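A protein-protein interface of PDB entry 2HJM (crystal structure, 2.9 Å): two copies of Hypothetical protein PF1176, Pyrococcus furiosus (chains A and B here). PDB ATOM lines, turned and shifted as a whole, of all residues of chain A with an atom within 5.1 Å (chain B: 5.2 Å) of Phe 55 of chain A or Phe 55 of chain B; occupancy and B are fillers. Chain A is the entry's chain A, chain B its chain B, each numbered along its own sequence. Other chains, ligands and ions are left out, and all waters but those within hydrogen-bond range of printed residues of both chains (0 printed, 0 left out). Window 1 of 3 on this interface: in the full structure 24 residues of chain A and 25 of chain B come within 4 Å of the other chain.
The backbone carbonyl oxygen of Glu 57 of chain A is in hydrogen-bond range of the side-chain hydroxyl of Thr 61 of chain A (3.2 Å).
Printed residues of chain B within 4 Å of Phe 55 of chain A: Gly 54 (3.2 Å), Phe 55 (3.99 Å), Glu 57 (3.99 Å), Gly 58 (3.4 Å) and Thr 61 (3.998 Å).
Of the printed residues of chain A, Phe 55 of chain B touches Gly 54, Phe 55, Glu 57 and Gly 58.
Printed residues of chain A within 4 Å of Ala 50 of chain B: Ser 51.
Printed residues of chain B within 4 Å of Ile 59 of chain A: Gly 58 (3.5 Å).
Of the printed residues of chain A, Thr 61 of chain B touches Ala 28 (3.8 Å) and Phe 55 (3.998 Å).
Printed residues of chain A within 4 Å of Ala 28 of chain B: Thr 61 (3.8 Å).
Of the printed residues of chain B, Phe 32 of chain A touches Glu 57 (3.7 Å).
Ile 29 of chain A touches none of the printed residues of chain B.
Ile 29 of chain B touches none of the printed residues of chain A.
The nearest printed residue of chain B that does not touch Phe 55 of chain A is Ser 51 of chain B (5.0 Å).
The nearest printed residue of chain B that does not touch Thr 61 of chain A is Phe 55 of chain B (4.3 Å).
Among the printed residues, pairs that only touch across the chains: Ala 28 of chain A with Thr 61 of chain B, Phe 32 of chain A with Glu 57 of chain B, Ala 50 of chain A with Ser 51 of chain B, Ser 51 of chain A with Ala 50 of chain B, Gly 54 of chain A with Ser 51 of chain B, Gly 54 of chain A with Phe 55 of chain B, Phe 55 of chain A with Gly 54 of chain B, Phe 55 of chain A with Phe 55 of chain B, Phe 55 of chain A with Glu 57 of chain B, Phe 55 of chain A with Gly 58 of chain B, Phe 55 of chain A with Thr 61 of chain B, Glu 57 of chain A with Phe 32 of chain B, Glu 57 of chain A with Phe 55 of chain B, Gly 58 of chain A with Phe 55 of chain B, Gly 58 of chain A with Gly 58 of chain B, Gly 58 of chain A with Ile 59 of chain B, Ile 59 of chain A with Gly 58 of chain B and Thr 61 of chain A with Ala 28 of chain B.
Printed residues of chain B that touch a printed residue of chain A: Ala 28, Phe 32, Ala 50, Ser 51, Gly 54, Phe 55, Glu 57, Gly 58, Ile 59 and Thr 61.
Hydrophobic or aromatic side chains of chain B within 4 Å of the printed part of chain A: Ala 28, Phe 32, Ala 50, Phe 55 and Ile 59.
Printed residues of chain A that touch a printed residue of chain B: Ala 28, Phe 32, Ala 50, Ser 51, Gly 54, Phe 55, Glu 57, Gly 58, Ile 59 and Thr 61.
Among the printed residues, no Asp or Glu carboxylate lies within 4 Å of a Lys or Arg side-chain nitrogen of the other chain.
Ala 28 of chain A touches Thr 61 of chain B, and with the chains exchanged Thr 61 of chain A touches Ala 28 of chain B.
Phe 32 of chain A touches Glu 57 of chain B, and with the chains exchanged Glu 57 of chain A touches Phe 32 of chain B.
Ala 50 of chain A touches Ser 51 of chain B, and with the chains exchanged Ser 51 of chain A touches Ala 50 of chain B.
Phe 55 of chain A touches its own counterpart, Phe 55 of chain B.
Positions printed for both chains: 28, 29, 32, 50, 51, 52, 53, 54, 55, 56, 57, 58, 59 and 61.
Of the 18 pairs that touch across the chains among the printed residues, 16 have their exchanged pair printed and touching as well.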
ATOM      1  N   ALA A  28       5.506 -26.148  23.543  1.00  0.00           N
ATOM      2  CA  ALA A  28       6.085 -25.934  22.212  1.00  0.00           C
ATOM      3  C   ALA A  28       7.535 -26.417  22.145  1.00  0.00           C
ATOM      4  O   ALA A  28       7.940 -27.066  21.176  1.00  0.00           O
ATOM      5  CB  ALA A  28       6.015 -24.463  21.853  1.00  0.00           C
ATOM      6  N   ILE A  29       8.319 -26.086  23.167  1.00  0.00           N
ATOM      7  CA  ILE A  29       9.707 -26.526  23.220  1.00  0.00           C
ATOM      8  C   ILE A  29       9.761 -28.038  23.026  1.00  0.00           C
ATOM      9  O   ILE A  29      10.416 -28.531  22.110  1.00  0.00           O
ATOM     10  CB  ILE A  29      10.361 -26.175  24.574  1.00  0.00           C
ATOM     11  CG1 ILE A  29      10.477 -24.658  24.708  1.00  0.00           C
ATOM     12  CG2 ILE A  29      11.732 -26.831  24.689  1.00  0.00           C
ATOM     13  CD1 ILE A  29      11.067 -24.194  26.035  1.00  0.00           C
ATOM     14  N   PHE A  32       9.277 -29.014  19.775  1.00  0.00           N
ATOM     15  CA  PHE A  32      10.468 -28.730  18.983  1.00  0.00           C
ATOM     16  C   PHE A  32      11.620 -29.728  19.226  1.00  0.00           C
ATOM     17  O   PHE A  32      12.153 -30.317  18.279  1.00  0.00           O
ATOM     18  CB  PHE A  32      10.938 -27.283  19.238  1.00  0.00           C
ATOM     19  CG  PHE A  32      12.094 -26.852  18.368  1.00  0.00           C
ATOM     20  CD1 PHE A  32      13.395 -27.242  18.664  1.00  0.00           C
ATOM     21  CD2 PHE A  32      11.871 -26.114  17.212  1.00  0.00           C
ATOM     22  CE1 PHE A  32      14.451 -26.911  17.823  1.00  0.00           C
ATOM     23  CE2 PHE A  32      12.924 -25.778  16.364  1.00  0.00           C
ATOM     24  CZ  PHE A  32      14.215 -26.180  16.673  1.00  0.00           C
ATOM     25  N   ALA A  50      22.954 -26.571  17.958  1.00  0.00           N
ATOM     26  CA  ALA A  50      22.868 -25.230  17.398  1.00  0.00           C
ATOM     27  C   ALA A  50      21.454 -24.879  17.009  1.00  0.00           C
ATOM     28  O   ALA A  50      21.078 -23.709  17.019  1.00  0.00           O
ATOM     29  CB  ALA A  50      23.775 -25.104  16.193  1.00  0.00           C
ATOM     30  N   SER A  51      20.662 -25.882  16.658  1.00  0.00           N
ATOM     31  CA  SER A  51      19.278 -25.620  16.294  1.00  0.00           C
ATOM     32  C   SER A  51      18.434 -25.417  17.555  1.00  0.00           C
ATOM     33  O   SER A  51      17.696 -24.440  17.678  1.00  0.00           O
ATOM     34  CB  SER A  51      18.715 -26.779  15.483  1.00  0.00           C
ATOM     35  OG  SER A  51      19.587 -27.114  14.416  1.00  0.00           O
ATOM     36  N   ILE A  52      18.554 -26.333  18.503  1.00  0.00           N
ATOM     37  CA  ILE A  52      17.784 -26.214  19.725  1.00  0.00           C
ATOM     38  C   ILE A  52      18.155 -24.952  20.495  1.00  0.00           C
ATOM     39  O   ILE A  52      17.274 -24.203  20.916  1.00  0.00           O
ATOM     40  CB  ILE A  52      17.999 -27.446  20.641  1.00  0.00           C
ATOM     41  CG1 ILE A  52      17.579 -28.720  19.911  1.00  0.00           C
ATOM     42  CG2 ILE A  52      17.174 -27.316  21.914  1.00  0.00           C
ATOM     43  CD1 ILE A  52      17.946 -29.974  20.661  1.00  0.00           C
ATOM     44  N   TYR A  53      19.456 -24.720  20.681  1.00  0.00           N
ATOM     45  CA  TYR A  53      19.936 -23.555  21.427  1.00  0.00           C
ATOM     46  C   TYR A  53      19.514 -22.257  20.774  1.00  0.00           C
ATOM     47  O   TYR A  53      19.070 -21.336  21.457  1.00  0.00           O
ATOM     48  CB  TYR A  53      21.463 -23.585  21.565  1.00  0.00           C
ATOM     49  CG  TYR A  53      21.986 -24.628  22.532  1.00  0.00           C
ATOM     50  CD1 TYR A  53      23.309 -25.048  22.475  1.00  0.00           C
ATOM     51  CD2 TYR A  53      21.149 -25.217  23.488  1.00  0.00           C
ATOM     52  CE1 TYR A  53      23.787 -26.032  23.338  1.00  0.00           C
ATOM     53  CE2 TYR A  53      21.617 -26.197  24.351  1.00  0.00           C
ATOM     54  CZ  TYR A  53      22.939 -26.602  24.272  1.00  0.00           C
ATOM     55  OH  TYR A  53      23.425 -27.575  25.122  1.00  0.00           O
ATOM     56  N   GLY A  54      19.659 -22.178  19.454  1.00  0.00           N
ATOM     57  CA  GLY A  54      19.258 -20.968  18.765  1.00  0.00           C
ATOM     58  C   GLY A  54      17.782 -20.739  19.021  1.00  0.00           C
ATOM     59  O   GLY A  54      17.324 -19.610  19.225  1.00  0.00           O
ATOM     60  N   PHE A  55      17.047 -21.845  19.010  1.00  0.00           N
ATOM     61  CA  PHE A  55      15.615 -21.858  19.240  1.00  0.00           C
ATOM     62  C   PHE A  55      15.293 -21.330  20.641  1.00  0.00           C
ATOM     63  O   PHE A  55      14.367 -20.539  20.824  1.00  0.00           O
ATOM     64  CB  PHE A  55      15.111 -23.287  19.066  1.00  0.00           C
ATOM     65  CG  PHE A  55      13.665 -23.464  19.377  1.00  0.00           C
ATOM     66  CD1 PHE A  55      13.269 -24.234  20.460  1.00  0.00           C
ATOM     67  CD2 PHE A  55      12.693 -22.870  18.593  1.00  0.00           C
ATOM     68  CE1 PHE A  55      11.916 -24.409  20.757  1.00  0.00           C
ATOM     69  CE2 PHE A  55      11.343 -23.040  18.886  1.00  0.00           C
ATOM     70  CZ  PHE A  55      10.954 -23.808  19.967  1.00  0.00           C
ATOM     71  N   LEU A  56      16.060 -21.757  21.632  1.00  0.00           N
ATOM     72  CA  LEU A  56      15.823 -21.292  22.982  1.00  0.00           C
ATOM     73  C   LEU A  56      16.137 -19.806  23.071  1.00  0.00           C
ATOM     74  O   LEU A  56      15.469 -19.073  23.801  1.00  0.00           O
ATOM     75  CB  LEU A  56      16.697 -22.053  23.976  1.00  0.00           C
ATOM     76  CG  LEU A  56      16.578 -23.573  24.041  1.00  0.00           C
ATOM     77  CD1 LEU A  56      17.502 -24.056  25.141  1.00  0.00           C
ATOM     78  CD2 LEU A  56      15.138 -24.007  24.307  1.00  0.00           C
ATOM     79  N   GLU A  57      17.163 -19.362  22.346  1.00  0.00           N
ATOM     80  CA  GLU A  57      17.535 -17.946  22.364  1.00  0.00           C
ATOM     81  C   GLU A  57      16.342 -17.162  21.886  1.00  0.00           C
ATOM     82  O   GLU A  57      15.913 -16.230  22.556  1.00  0.00           O
ATOM     83  CB  GLU A  57      18.744 -17.652  21.460  1.00  0.00           C
ATOM     84  CG  GLU A  57      20.057 -17.479  22.228  1.00  0.00           C
ATOM     85  CD  GLU A  57      21.022 -16.472  21.594  1.00  0.00           C
ATOM     86  OE1 GLU A  57      20.600 -15.343  21.265  1.00  0.00           O
ATOM     87  OE2 GLU A  57      22.213 -16.798  21.442  1.00  0.00           O
ATOM     88  N   GLY A  58      15.812 -17.556  20.727  1.00  0.00           N
ATOM     89  CA  GLY A  58      14.645 -16.903  20.166  1.00  0.00           C
ATOM     90  C   GLY A  58      13.521 -16.830  21.189  1.00  0.00           C
ATOM     91  O   GLY A  58      12.876 -15.804  21.334  1.00  0.00           O
ATOM     92  N   ILE A  59      13.267 -17.913  21.907  1.00  0.00           N
ATOM     93  CA  ILE A  59      12.230 -17.881  22.920  1.00  0.00           C
ATOM     94  C   ILE A  59      12.621 -16.900  24.038  1.00  0.00           C
ATOM     95  O   ILE A  59      11.909 -15.930  24.312  1.00  0.00           O
ATOM     96  CB  ILE A  59      12.008 -19.279  23.505  1.00  0.00           C
ATOM     97  CG1 ILE A  59      11.201 -20.117  22.512  1.00  0.00           C
ATOM     98  CG2 ILE A  59      11.305 -19.184  24.846  1.00  0.00           C
ATOM     99  CD1 ILE A  59      11.076 -21.586  22.883  1.00  0.00           C
ATOM    100  N   THR A  61      14.550 -14.508  24.100  1.00  0.00           N
ATOM    101  CA  THR A  61      14.662 -13.115  23.682  1.00  0.00           C
ATOM    102  C   THR A  61      13.325 -12.419  23.547  1.00  0.00           C
ATOM    103  O   THR A  61      13.184 -11.276  23.983  1.00  0.00           O
ATOM    104  CB  THR A  61      15.449 -12.970  22.361  1.00  0.00           C
ATOM    105  OG1 THR A  61      16.837 -13.211  22.611  1.00  0.00           O
ATOM    106  CG2 THR A  61      15.304 -11.567  21.791  1.00  0.00           C
ATOM    107  N   ALA B  28      17.235  -7.241  17.957  1.00  0.00           N
ATOM    108  CA  ALA B  28      17.870  -8.478  18.398  1.00  0.00           C
ATOM    109  C   ALA B  28      18.213  -9.330  17.180  1.00  0.00           C
ATOM    110  O   ALA B  28      19.362  -9.728  16.992  1.00  0.00           O
ATOM    111  CB  ALA B  28      16.946  -9.235  19.326  1.00  0.00           C
ATOM    112  N   ILE B  29      17.212  -9.609  16.353  1.00  0.00           N
ATOM    113  CA  ILE B  29      17.435 -10.398  15.154  1.00  0.00           C
ATOM    114  C   ILE B  29      18.642  -9.822  14.438  1.00  0.00           C
ATOM    115  O   ILE B  29      19.504 -10.543  13.955  1.00  0.00           O
ATOM    116  CB  ILE B  29      16.211 -10.336  14.220  1.00  0.00           C
ATOM    117  CG1 ILE B  29      15.013 -10.981  14.914  1.00  0.00           C
ATOM    118  CG2 ILE B  29      16.512 -11.019  12.893  1.00  0.00           C
ATOM    119  CD1 ILE B  29      13.733 -10.946  14.098  1.00  0.00           C
ATOM    120  N   PHE B  32      21.729 -10.695  16.327  1.00  0.00           N
ATOM    121  CA  PHE B  32      21.949 -12.132  16.315  1.00  0.00           C
ATOM    122  C   PHE B  32      22.659 -12.455  15.013  1.00  0.00           C
ATOM    123  O   PHE B  32      23.729 -13.059  15.002  1.00  0.00           O
ATOM    124  CB  PHE B  32      20.617 -12.908  16.419  1.00  0.00           C
ATOM    125  CG  PHE B  32      20.797 -14.411  16.550  1.00  0.00           C
ATOM    126  CD1 PHE B  32      20.873 -15.221  15.422  1.00  0.00           C
ATOM    127  CD2 PHE B  32      21.003 -14.993  17.796  1.00  0.00           C
ATOM    128  CE1 PHE B  32      21.159 -16.578  15.534  1.00  0.00           C
ATOM    129  CE2 PHE B  32      21.287 -16.341  17.912  1.00  0.00           C
ATOM    130  CZ  PHE B  32      21.368 -17.134  16.781  1.00  0.00           C
ATOM    131  N   ALA B  50      20.580 -23.300  10.124  1.00  0.00           N
ATOM    132  CA  ALA B  50      19.810 -24.001  11.142  1.00  0.00           C
ATOM    133  C   ALA B  50      19.753 -23.226  12.460  1.00  0.00           C
ATOM    134  O   ALA B  50      18.752 -23.287  13.170  1.00  0.00           O
ATOM    135  CB  ALA B  50      20.392 -25.394  11.375  1.00  0.00           C
ATOM    136  N   SER B  51      20.821 -22.505  12.786  1.00  0.00           N
ATOM    137  CA  SER B  51      20.857 -21.726  14.022  1.00  0.00           C
ATOM    138  C   SER B  51      19.953 -20.496  13.932  1.00  0.00           C
ATOM    139  O   SER B  51      19.175 -20.199  14.853  1.00  0.00           O
ATOM    140  CB  SER B  51      22.275 -21.238  14.313  1.00  0.00           C
ATOM    141  OG  SER B  51      23.201 -22.300  14.284  1.00  0.00           O
ATOM    142  N   ILE B  52      20.089 -19.777  12.817  1.00  0.00           N
ATOM    143  CA  ILE B  52      19.323 -18.569  12.560  1.00  0.00           C
ATOM    144  C   ILE B  52      17.838 -18.864  12.416  1.00  0.00           C
ATOM    145  O   ILE B  52      17.002 -18.121  12.939  1.00  0.00           O
ATOM    146  CB  ILE B  52      19.834 -17.874  11.282  1.00  0.00           C
ATOM    147  CG1 ILE B  52      21.289 -17.463  11.487  1.00  0.00           C
ATOM    148  CG2 ILE B  52      18.966 -16.663  10.944  1.00  0.00           C
ATOM    149  CD1 ILE B  52      21.890 -16.750  10.306  1.00  0.00           C
ATOM    150  N   TYR B  53      17.516 -19.942  11.703  1.00  0.00           N
ATOM    151  CA  TYR B  53      16.125 -20.335  11.513  1.00  0.00           C
ATOM    152  C   TYR B  53      15.530 -20.811  12.838  1.00  0.00           C
ATOM    153  O   TYR B  53      14.400 -20.462  13.184  1.00  0.00           O
ATOM    154  CB  TYR B  53      16.017 -21.447  10.471  1.00  0.00           C
ATOM    155  CG  TYR B  53      16.293 -21.023   9.041  1.00  0.00           C
ATOM    156  CD1 TYR B  53      16.643 -21.966   8.070  1.00  0.00           C
ATOM    157  CD2 TYR B  53      16.214 -19.688   8.657  1.00  0.00           C
ATOM    158  CE1 TYR B  53      16.912 -21.584   6.758  1.00  0.00           C
ATOM    159  CE2 TYR B  53      16.479 -19.300   7.347  1.00  0.00           C
ATOM    160  CZ  TYR B  53      16.828 -20.249   6.406  1.00  0.00           C
ATOM    161  OH  TYR B  53      17.100 -19.860   5.116  1.00  0.00           O
ATOM    162  N   GLY B  54      16.282 -21.614  13.581  1.00  0.00           N
ATOM    163  CA  GLY B  54      15.779 -22.073  14.859  1.00  0.00           C
ATOM    164  C   GLY B  54      15.505 -20.848  15.708  1.00  0.00           C
ATOM    165  O   GLY B  54      14.518 -20.773  16.443  1.00  0.00           O
ATOM    166  N   PHE B  55      16.401 -19.876  15.595  1.00  0.00           N
ATOM    167  CA  PHE B  55      16.275 -18.629  16.327  1.00  0.00           C
ATOM    168  C   PHE B  55      14.986 -17.924  15.927  1.00  0.00           C
ATOM    169  O   PHE B  55      14.225 -17.472  16.777  1.00  0.00           O
ATOM    170  CB  PHE B  55      17.468 -17.717  16.040  1.00  0.00           C
ATOM    171  CG  PHE B  55      17.414 -16.416  16.777  1.00  0.00           C
ATOM    172  CD1 PHE B  55      17.180 -15.221  16.095  1.00  0.00           C
ATOM    173  CD2 PHE B  55      17.564 -16.384  18.164  1.00  0.00           C
ATOM    174  CE1 PHE B  55      17.093 -14.008  16.783  1.00  0.00           C
ATOM    175  CE2 PHE B  55      17.482 -15.187  18.863  1.00  0.00           C
ATOM    176  CZ  PHE B  55      17.245 -13.995  18.172  1.00  0.00           C
ATOM    177  N   LEU B  56      14.750 -17.827  14.627  1.00  0.00           N
ATOM    178  CA  LEU B  56      13.550 -17.184  14.124  1.00  0.00           C
ATOM    179  C   LEU B  56      12.284 -17.919  14.573  1.00  0.00           C
ATOM    180  O   LEU B  56      11.290 -17.279  14.942  1.00  0.00           O
ATOM    181  CB  LEU B  56      13.593 -17.123  12.598  1.00  0.00           C
ATOM    182  CG  LEU B  56      14.621 -16.157  12.027  1.00  0.00           C
ATOM    183  CD1 LEU B  56      14.637 -16.242  10.515  1.00  0.00           C
ATOM    184  CD2 LEU B  56      14.267 -14.747  12.478  1.00  0.00           C
ATOM    185  N   GLU B  57      12.316 -19.254  14.536  1.00  0.00           N
ATOM    186  CA  GLU B  57      11.154 -20.024  14.946  1.00  0.00           C
ATOM    187  C   GLU B  57      10.914 -19.886  16.435  1.00  0.00           C
ATOM    188  O   GLU B  57       9.779 -19.957  16.893  1.00  0.00           O
ATOM    189  CB  GLU B  57      11.298 -21.501  14.606  1.00  0.00           C
ATOM    190  CG  GLU B  57      10.054 -22.265  15.026  1.00  0.00           C
ATOM    191  CD  GLU B  57      10.036 -23.728  14.619  1.00  0.00           C
ATOM    192  OE1 GLU B  57       9.158 -24.455  15.139  1.00  0.00           O
ATOM    193  OE2 GLU B  57      10.870 -24.155  13.787  1.00  0.00           O
ATOM    194  N   GLY B  58      11.990 -19.699  17.191  1.00  0.00           N
ATOM    195  CA  GLY B  58      11.853 -19.531  18.622  1.00  0.00           C
ATOM    196  C   GLY B  58      11.069 -18.262  18.889  1.00  0.00           C
ATOM    197  O   GLY B  58      10.248 -18.210  19.798  1.00  0.00           O
ATOM    198  N   ILE B  59      11.328 -17.234  18.089  1.00  0.00           N
ATOM    199  CA  ILE B  59      10.644 -15.965  18.214  1.00  0.00           C
ATOM    200  C   ILE B  59       9.212 -16.123  17.705  1.00  0.00           C
ATOM    201  O   ILE B  59       8.249 -15.895  18.438  1.00  0.00           O
ATOM    202  CB  ILE B  59      11.358 -14.892  17.384  1.00  0.00           C
ATOM    203  CG1 ILE B  59      12.821 -14.814  17.812  1.00  0.00           C
ATOM    204  CG2 ILE B  59      10.668 -13.542  17.551  1.00  0.00           C
ATOM    205  CD1 ILE B  59      13.649 -13.880  16.973  1.00  0.00           C
ATOM    206  N   THR B  61       7.442 -18.485  17.476  1.00  0.00           N
ATOM    207  CA  THR B  61       6.679 -19.369  18.342  1.00  0.00           C
ATOM    208  C   THR B  61       6.146 -18.665  19.572  1.00  0.00           C
ATOM    209  O   THR B  61       4.949 -18.711  19.857  1.00  0.00           O
ATOM    210  CB  THR B  61       7.523 -20.544  18.809  1.00  0.00           C
ATOM    211  OG1 THR B  61       7.959 -21.291  17.671  1.00  0.00           O
ATOM    212  CG2 THR B  61       6.712 -21.454  19.724  1.00  0.00           C
